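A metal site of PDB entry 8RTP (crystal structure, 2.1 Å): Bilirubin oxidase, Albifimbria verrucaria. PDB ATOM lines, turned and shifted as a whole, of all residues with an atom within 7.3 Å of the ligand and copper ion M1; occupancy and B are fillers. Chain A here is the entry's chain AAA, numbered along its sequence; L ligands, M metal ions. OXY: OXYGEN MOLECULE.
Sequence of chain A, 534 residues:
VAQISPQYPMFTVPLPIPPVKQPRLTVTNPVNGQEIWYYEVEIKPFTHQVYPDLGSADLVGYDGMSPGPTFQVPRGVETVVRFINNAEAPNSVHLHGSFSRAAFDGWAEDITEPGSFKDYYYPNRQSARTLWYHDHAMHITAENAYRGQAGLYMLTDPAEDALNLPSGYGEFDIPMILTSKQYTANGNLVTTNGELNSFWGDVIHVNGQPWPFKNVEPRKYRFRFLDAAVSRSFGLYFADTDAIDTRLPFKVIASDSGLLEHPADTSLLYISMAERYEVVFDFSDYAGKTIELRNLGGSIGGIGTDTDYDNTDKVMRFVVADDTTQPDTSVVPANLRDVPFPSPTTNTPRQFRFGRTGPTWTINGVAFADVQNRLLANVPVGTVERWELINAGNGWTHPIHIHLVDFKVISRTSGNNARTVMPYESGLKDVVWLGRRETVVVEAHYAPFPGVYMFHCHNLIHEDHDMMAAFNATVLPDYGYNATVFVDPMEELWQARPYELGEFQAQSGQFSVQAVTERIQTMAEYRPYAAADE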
ATOM      1  N   HIS A  94     -11.041   4.132 -30.019  1.00  0.00           N
ATOM      2  CA  HIS A  94     -10.621   2.720 -29.924  1.00  0.00           C
ATOM      3  C   HIS A  94     -11.863   1.815 -29.820  1.00  0.00           C
ATOM      4  O   HIS A  94     -12.712   1.982 -28.846  1.00  0.00           O
ATOM      5  CB  HIS A  94      -9.715   2.551 -28.707  1.00  0.00           C
ATOM      6  CG  HIS A  94      -9.354   1.147 -28.483  1.00  0.00           C
ATOM      7  ND1 HIS A  94      -8.854   0.336 -29.501  1.00  0.00           N
ATOM      8  CD2 HIS A  94      -9.417   0.384 -27.377  1.00  0.00           C
ATOM      9  CE1 HIS A  94      -8.584  -0.847 -29.012  1.00  0.00           C
ATOM     10  NE2 HIS A  94      -8.925  -0.838 -27.717  1.00  0.00           N
ATOM     11  N   LEU A  95     -11.963   0.874 -30.747  1.00  0.00           N
ATOM     12  CA  LEU A  95     -12.884  -0.279 -30.627  1.00  0.00           C
ATOM     13  C   LEU A  95     -12.184  -1.371 -29.833  1.00  0.00           C
ATOM     14  O   LEU A  95     -11.400  -2.112 -30.437  1.00  0.00           O
ATOM     15  CB  LEU A  95     -13.245  -0.810 -32.013  1.00  0.00           C
ATOM     16  CG  LEU A  95     -14.320  -1.884 -31.993  1.00  0.00           C
ATOM     17  CD1 LEU A  95     -15.564  -1.382 -31.240  1.00  0.00           C
ATOM     18  CD2 LEU A  95     -14.660  -2.318 -33.411  1.00  0.00           C
ATOM     19  N   HIS A  96     -12.453  -1.429 -28.529  1.00  0.00           N
ATOM     20  CA  HIS A  96     -11.808  -2.335 -27.575  1.00  0.00           C
ATOM     21  C   HIS A  96     -12.445  -3.728 -27.732  1.00  0.00           C
ATOM     22  O   HIS A  96     -13.672  -3.848 -27.624  1.00  0.00           O
ATOM     23  CB  HIS A  96     -11.902  -1.698 -26.194  1.00  0.00           C
ATOM     24  CG  HIS A  96     -11.156  -2.458 -25.147  1.00  0.00           C
ATOM     25  ND1 HIS A  96     -10.567  -1.820 -24.087  1.00  0.00           N
ATOM     26  CD2 HIS A  96     -10.951  -3.771 -24.954  1.00  0.00           C
ATOM     27  CE1 HIS A  96     -10.018  -2.714 -23.286  1.00  0.00           C
ATOM     28  NE2 HIS A  96     -10.246  -3.923 -23.799  1.00  0.00           N
ATOM     29  N   ASP A 105      -7.324   1.794 -34.777  1.00  0.00           N
ATOM     30  CA  ASP A 105      -7.311   1.142 -33.449  1.00  0.00           C
ATOM     31  C   ASP A 105      -7.379   2.155 -32.322  1.00  0.00           C
ATOM     32  O   ASP A 105      -7.454   1.701 -31.156  1.00  0.00           O
ATOM     33  CB  ASP A 105      -6.085   0.240 -33.250  1.00  0.00           C
ATOM     34  CG  ASP A 105      -6.251  -0.716 -32.092  1.00  0.00           C
ATOM     35  OD1 ASP A 105      -7.353  -1.324 -32.050  1.00  0.00           O
ATOM     36  OD2 ASP A 105      -5.322  -0.790 -31.188  1.00  0.00           O
ATOM     37  N   GLY A 106      -7.417   3.470 -32.634  1.00  0.00           N
ATOM     38  CA  GLY A 106      -7.480   4.546 -31.614  1.00  0.00           C
ATOM     39  C   GLY A 106      -6.145   4.791 -30.941  1.00  0.00           C
ATOM     40  O   GLY A 106      -6.136   5.144 -29.774  1.00  0.00           O
ATOM     41  N   TRP A 132     -16.504  -2.594 -26.858  1.00  0.00           N
ATOM     42  CA  TRP A 132     -16.970  -1.237 -26.549  1.00  0.00           C
ATOM     43  C   TRP A 132     -16.046  -0.271 -27.262  1.00  0.00           C
ATOM     44  O   TRP A 132     -14.882  -0.665 -27.547  1.00  0.00           O
ATOM     45  CB  TRP A 132     -17.100  -1.005 -25.041  1.00  0.00           C
ATOM     46  CG  TRP A 132     -15.852  -1.071 -24.221  1.00  0.00           C
ATOM     47  CD1 TRP A 132     -14.927  -2.073 -24.135  1.00  0.00           C
ATOM     48  CD2 TRP A 132     -15.413  -0.047 -23.312  1.00  0.00           C
ATOM     49  NE1 TRP A 132     -13.948  -1.746 -23.221  1.00  0.00           N
ATOM     50  CE2 TRP A 132     -14.211  -0.492 -22.719  1.00  0.00           C
ATOM     51  CE3 TRP A 132     -15.931   1.189 -22.931  1.00  0.00           C
ATOM     52  CZ2 TRP A 132     -13.534   0.271 -21.777  1.00  0.00           C
ATOM     53  CZ3 TRP A 132     -15.233   1.951 -22.003  1.00  0.00           C
ATOM     54  CH2 TRP A 132     -14.071   1.475 -21.416  1.00  0.00           C
ATOM     55  N   HIS A 134     -14.641   3.699 -27.343  1.00  0.00           N
ATOM     56  CA  HIS A 134     -14.416   4.751 -26.328  1.00  0.00           C
ATOM     57  C   HIS A 134     -13.247   5.634 -26.752  1.00  0.00           C
ATOM     58  O   HIS A 134     -12.373   5.201 -27.557  1.00  0.00           O
ATOM     59  CB  HIS A 134     -14.258   4.131 -24.934  1.00  0.00           C
ATOM     60  CG  HIS A 134     -12.976   3.382 -24.730  1.00  0.00           C
ATOM     61  ND1 HIS A 134     -11.748   4.031 -24.614  1.00  0.00           N
ATOM     62  CD2 HIS A 134     -12.734   2.074 -24.583  1.00  0.00           C
ATOM     63  CE1 HIS A 134     -10.809   3.138 -24.415  1.00  0.00           C
ATOM     64  NE2 HIS A 134     -11.382   1.927 -24.376  1.00  0.00           N
ATOM     65  N   ASP A 135     -13.162   6.800 -26.149  1.00  0.00           N
ATOM     66  CA  ASP A 135     -12.049   7.718 -26.456  1.00  0.00           C
ATOM     67  C   ASP A 135     -10.709   7.172 -25.952  1.00  0.00           C
ATOM     68  O   ASP A 135     -10.642   6.417 -24.904  1.00  0.00           O
ATOM     69  CB  ASP A 135     -12.283   9.105 -25.878  1.00  0.00           C
ATOM     70  CG  ASP A 135     -11.309  10.042 -26.545  1.00  0.00           C
ATOM     71  OD1 ASP A 135     -11.469  10.234 -27.783  1.00  0.00           O
ATOM     72  OD2 ASP A 135     -10.356  10.493 -25.829  1.00  0.00           O
ATOM     73  N   HIS A 136      -9.647   7.539 -26.655  1.00  0.00           N
ATOM     74  CA  HIS A 136      -8.274   7.113 -26.326  1.00  0.00           C
ATOM     75  C   HIS A 136      -7.247   8.229 -26.570  1.00  0.00           C
ATOM     76  O   HIS A 136      -6.071   7.922 -26.578  1.00  0.00           O
ATOM     77  CB  HIS A 136      -7.993   5.866 -27.149  1.00  0.00           C
ATOM     78  CG  HIS A 136      -7.131   4.883 -26.456  1.00  0.00           C
ATOM     79  ND1 HIS A 136      -5.877   5.224 -25.994  1.00  0.00           N
ATOM     80  CD2 HIS A 136      -7.331   3.570 -26.174  1.00  0.00           C
ATOM     81  CE1 HIS A 136      -5.338   4.161 -25.414  1.00  0.00           C
ATOM     82  NE2 HIS A 136      -6.204   3.126 -25.538  1.00  0.00           N
ATOM     83  N   THR A 141      -7.883  10.950 -22.235  1.00  0.00           N
ATOM     84  CA  THR A 141      -8.766   9.750 -22.288  1.00  0.00           C
ATOM     85  C   THR A 141      -9.696   9.714 -21.066  1.00  0.00           C
ATOM     86  O   THR A 141     -10.897   9.431 -21.225  1.00  0.00           O
ATOM     87  CB  THR A 141      -7.933   8.464 -22.431  1.00  0.00           C
ATOM     88  OG1 THR A 141      -7.318   8.521 -23.709  1.00  0.00           O
ATOM     89  CG2 THR A 141      -8.750   7.194 -22.325  1.00  0.00           C
ATOM     90  N   ALA A 274     -12.404  -1.826 -18.017  1.00  0.00           N
ATOM     91  CA  ALA A 274     -12.404  -2.234 -19.441  1.00  0.00           C
ATOM     92  C   ALA A 274     -12.729  -3.718 -19.579  1.00  0.00           C
ATOM     93  O   ALA A 274     -12.823  -4.177 -20.719  1.00  0.00           O
ATOM     94  CB  ALA A 274     -11.108  -1.903 -20.126  1.00  0.00           C
ATOM     95  N   HIS A 401      -4.424  -3.736 -20.247  1.00  0.00           N
ATOM     96  CA  HIS A 401      -5.003  -3.992 -21.578  1.00  0.00           C
ATOM     97  C   HIS A 401      -3.892  -4.064 -22.619  1.00  0.00           C
ATOM     98  O   HIS A 401      -2.993  -3.166 -22.667  1.00  0.00           O
ATOM     99  CB  HIS A 401      -6.067  -2.921 -21.835  1.00  0.00           C
ATOM    100  CG  HIS A 401      -6.639  -3.070 -23.192  1.00  0.00           C
ATOM    101  ND1 HIS A 401      -6.980  -4.297 -23.717  1.00  0.00           N
ATOM    102  CD2 HIS A 401      -6.870  -2.162 -24.151  1.00  0.00           C
ATOM    103  CE1 HIS A 401      -7.429  -4.126 -24.933  1.00  0.00           C
ATOM    104  NE2 HIS A 401      -7.364  -2.827 -25.223  1.00  0.00           N
ATOM    105  N   ILE A 402      -3.898  -5.134 -23.402  1.00  0.00           N
ATOM    106  CA  ILE A 402      -3.017  -5.335 -24.585  1.00  0.00           C
ATOM    107  C   ILE A 402      -3.924  -5.253 -25.833  1.00  0.00           C
ATOM    108  O   ILE A 402      -4.845  -6.069 -25.988  1.00  0.00           O
ATOM    109  CB  ILE A 402      -2.201  -6.638 -24.485  1.00  0.00           C
ATOM    110  CG1 ILE A 402      -1.622  -6.845 -23.085  1.00  0.00           C
ATOM    111  CG2 ILE A 402      -1.141  -6.670 -25.557  1.00  0.00           C
ATOM    112  CD1 ILE A 402      -0.852  -8.147 -22.871  1.00  0.00           C
ATOM    113  N   HIS A 403      -3.703  -4.236 -26.655  1.00  0.00           N
ATOM    114  CA  HIS A 403      -4.354  -4.078 -27.976  1.00  0.00           C
ATOM    115  C   HIS A 403      -3.970  -5.245 -28.892  1.00  0.00           C
ATOM    116  O   HIS A 403      -2.998  -5.938 -28.571  1.00  0.00           O
ATOM    117  CB  HIS A 403      -3.935  -2.739 -28.548  1.00  0.00           C
ATOM    118  CG  HIS A 403      -4.627  -1.583 -27.925  1.00  0.00           C
ATOM    119  ND1 HIS A 403      -5.337  -0.681 -28.679  1.00  0.00           N
ATOM    120  CD2 HIS A 403      -4.641  -1.114 -26.648  1.00  0.00           C
ATOM    121  CE1 HIS A 403      -5.816   0.260 -27.885  1.00  0.00           C
ATOM    122  NE2 HIS A 403      -5.388   0.037 -26.653  1.00  0.00           N
ATOM    123  N   VAL A 431      -7.976  -7.768 -21.100  1.00  0.00           N
ATOM    124  CA  VAL A 431      -7.681  -6.976 -19.879  1.00  0.00           C
ATOM    125  C   VAL A 431      -7.515  -7.944 -18.708  1.00  0.00           C
ATOM    126  O   VAL A 431      -8.271  -8.959 -18.583  1.00  0.00           O
ATOM    127  CB  VAL A 431      -8.805  -5.968 -19.592  1.00  0.00           C
ATOM    128  CG1 VAL A 431      -8.536  -5.220 -18.319  1.00  0.00           C
ATOM    129  CG2 VAL A 431      -8.977  -4.987 -20.737  1.00  0.00           C
ATOM    130  N   MET A 454      -0.715  -0.206 -28.770  1.00  0.00           N
ATOM    131  CA  MET A 454      -0.569   0.167 -27.347  1.00  0.00           C
ATOM    132  C   MET A 454      -0.876  -1.015 -26.423  1.00  0.00           C
ATOM    133  O   MET A 454      -1.632  -1.910 -26.801  1.00  0.00           O
ATOM    134  CB  MET A 454      -1.539   1.302 -27.025  1.00  0.00           C
ATOM    135  CG  MET A 454      -1.159   2.536 -27.812  1.00  0.00           C
ATOM    136  SD  MET A 454      -2.372   3.836 -27.675  1.00  0.00           S
ATOM    137  CE  MET A 454      -3.884   3.014 -28.233  1.00  0.00           C
ATOM    138  N   PHE A 455      -0.270  -0.973 -25.259  1.00  0.00           N
ATOM    139  CA  PHE A 455      -0.682  -1.722 -24.056  1.00  0.00           C
ATOM    140  C   PHE A 455      -0.499  -0.781 -22.873  1.00  0.00           C
ATOM    141  O   PHE A 455       0.339   0.154 -22.909  1.00  0.00           O
ATOM    142  CB  PHE A 455       0.062  -3.058 -24.001  1.00  0.00           C
ATOM    143  CG  PHE A 455       1.513  -3.001 -23.594  1.00  0.00           C
ATOM    144  CD1 PHE A 455       2.482  -2.660 -24.529  1.00  0.00           C
ATOM    145  CD2 PHE A 455       1.886  -3.326 -22.305  1.00  0.00           C
ATOM    146  CE1 PHE A 455       3.829  -2.677 -24.167  1.00  0.00           C
ATOM    147  CE2 PHE A 455       3.216  -3.327 -21.945  1.00  0.00           C
ATOM    148  CZ  PHE A 455       4.190  -3.020 -22.872  1.00  0.00           C
ATOM    149  N   HIS A 456      -1.338  -0.941 -21.869  1.00  0.00           N
ATOM    150  CA  HIS A 456      -1.433   0.070 -20.803  1.00  0.00           C
ATOM    151  C   HIS A 456      -2.316  -0.433 -19.681  1.00  0.00           C
ATOM    152  O   HIS A 456      -3.134  -1.429 -19.862  1.00  0.00           O
ATOM    153  CB  HIS A 456      -1.978   1.373 -21.403  1.00  0.00           C
ATOM    154  CG  HIS A 456      -3.315   1.232 -22.049  1.00  0.00           C
ATOM    155  ND1 HIS A 456      -4.484   1.464 -21.350  1.00  0.00           N
ATOM    156  CD2 HIS A 456      -3.666   0.921 -23.314  1.00  0.00           C
ATOM    157  CE1 HIS A 456      -5.511   1.287 -22.150  1.00  0.00           C
ATOM    158  NE2 HIS A 456      -5.039   0.940 -23.361  1.00  0.00           N
ATOM    159  N   CYS A 457      -2.176   0.250 -18.563  1.00  0.00           N
ATOM    160  CA  CYS A 457      -3.212   0.216 -17.529  1.00  0.00           C
ATOM    161  C   CYS A 457      -4.482   0.917 -18.030  1.00  0.00           C
ATOM    162  O   CYS A 457      -4.384   2.018 -18.633  1.00  0.00           O
ATOM    163  CB  CYS A 457      -2.654   0.817 -16.253  1.00  0.00           C
ATOM    164  SG  CYS A 457      -3.888   0.824 -14.940  1.00  0.00           S
ATOM    165  N   HIS A 458      -5.645   0.381 -17.664  1.00  0.00           N
ATOM    166  CA  HIS A 458      -6.960   0.922 -18.067  1.00  0.00           C
ATOM    167  C   HIS A 458      -7.559   1.666 -16.908  1.00  0.00           C
ATOM    168  O   HIS A 458      -8.739   2.099 -17.015  1.00  0.00           O
ATOM    169  CB  HIS A 458      -7.886  -0.194 -18.598  1.00  0.00           C
ATOM    170  CG  HIS A 458      -8.714   0.241 -19.740  1.00  0.00           C
ATOM    171  ND1 HIS A 458      -9.680   1.218 -19.626  1.00  0.00           N
ATOM    172  CD2 HIS A 458      -8.674  -0.095 -21.047  1.00  0.00           C
ATOM    173  CE1 HIS A 458     -10.244   1.427 -20.802  1.00  0.00           C
ATOM    174  NE2 HIS A 458      -9.628   0.646 -21.696  1.00  0.00           N
ATOM    175  N   LEU A 460      -7.859   4.984 -16.170  1.00  0.00           N
ATOM    176  CA  LEU A 460      -7.729   6.095 -17.159  1.00  0.00           C
ATOM    177  C   LEU A 460      -6.875   7.252 -16.592  1.00  0.00           C
ATOM    178  O   LEU A 460      -6.217   7.937 -17.413  1.00  0.00           O
ATOM    179  CB  LEU A 460      -9.112   6.559 -17.613  1.00  0.00           C
ATOM    180  CG  LEU A 460     -10.005   5.495 -18.258  1.00  0.00           C
ATOM    181  CD1 LEU A 460     -11.245   6.150 -18.791  1.00  0.00           C
ATOM    182  CD2 LEU A 460      -9.304   4.717 -19.367  1.00  0.00           C
ATOM    183  N   GLU A 463      -3.398   5.737 -17.060  1.00  0.00           N
ATOM    184  CA  GLU A 463      -3.234   5.706 -18.511  1.00  0.00           C
ATOM    185  C   GLU A 463      -2.740   7.071 -19.019  1.00  0.00           C
ATOM    186  O   GLU A 463      -1.791   7.126 -19.819  1.00  0.00           O
ATOM    187  CB  GLU A 463      -4.576   5.362 -19.144  1.00  0.00           C
ATOM    188  CG  GLU A 463      -4.491   5.223 -20.644  1.00  0.00           C
ATOM    189  CD  GLU A 463      -5.686   4.574 -21.343  1.00  0.00           C
ATOM    190  OE1 GLU A 463      -6.426   3.793 -20.664  1.00  0.00           O
ATOM    191  OE2 GLU A 463      -5.895   4.911 -22.554  1.00  0.00           O
ATOM    192  N   MET A 468       1.439   3.667 -20.151  1.00  0.00           N
ATOM    193  CA  MET A 468       1.093   3.164 -21.487  1.00  0.00           C
ATOM    194  C   MET A 468       2.396   3.088 -22.255  1.00  0.00           C
ATOM    195  O   MET A 468       3.275   3.956 -22.043  1.00  0.00           O
ATOM    196  CB  MET A 468       0.106   4.120 -22.171  1.00  0.00           C
ATOM    197  CG  MET A 468      -0.464   3.649 -23.495  1.00  0.00           C
ATOM    198  SD  MET A 468      -2.075   4.446 -23.871  1.00  0.00           S
ATOM    199  CE  MET A 468      -1.513   6.080 -24.335  1.00  0.00           C
HETATM  200  O1  OXY L   1      -7.805   0.531 -24.579  1.00  0.00           O
HETATM  201  O2  OXY L   1      -8.242   1.532 -24.080  1.00  0.00           O
HETATM  202 CU    CU M   1      -5.959   1.231 -25.154  1.00  0.00          CU
HETATM  203 CU    CU M   2     -10.505   0.205 -23.706  1.00  0.00          CU
HETATM  204 CU    CU M   3      -8.176  -1.797 -26.420  1.00  0.00          CU
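The backbone carbonyl oxygen (O) of His 136 lies close to the side-chain hydroxyl (OG1) of Thr 141 (3.2 Å). A ring nitrogen (ND1) of His 94 lies within hydrogen-bond range of the backbone carbonyl oxygen of Asp 105, 2.6 Å away. A ring nitrogen (ND1) of His 136 sits close to the side-chain carboxylate (OE2) of Glu 463. The backbone NH (N) of His 134 lies within hydrogen-bond range of the backbone carbonyl oxygen (O) of His 94 (3.0 Å). ND1 of His 456 lies close to OE1 of Glu 463 (3.1 Å). N of His 403 lies close to O of Met 454 (3.1 Å). ND1 of His 401 sits close to NE2 of His 96, 3.3 Å away. The backbone carbonyl oxygen of His 456 lies within hydrogen-bond range of the backbone NH of His 401 (2.7 Å).
Merely in contact with copper ion M1: His 401 (3.7 Å).
NE2 of His 134 sits close to O2 of the ligand. NE2 of His 401 sits close to O1 of the ligand, at 3.4 Å. NE2 of His 458 sits close to O2 of the ligand (2.9 Å). His 94 touches the ligand (CD2 to O1, 3.2 Å). His 96 touches the ligand. Hydrophobic or aromatic side chains that line the ligand: His 94, His 134, His 136, His 401, His 403, His 456 and His 458. Of the 23 residues printed, 8 come within 4 Å of the ligand.
Copper ion M1 is bound by NE2 of His 136 (1.9 Å), NE2 of His 403 (2.0 Å), NE2 of His 456 (2.0 Å) and O1 of the ligand (2.1 Å).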
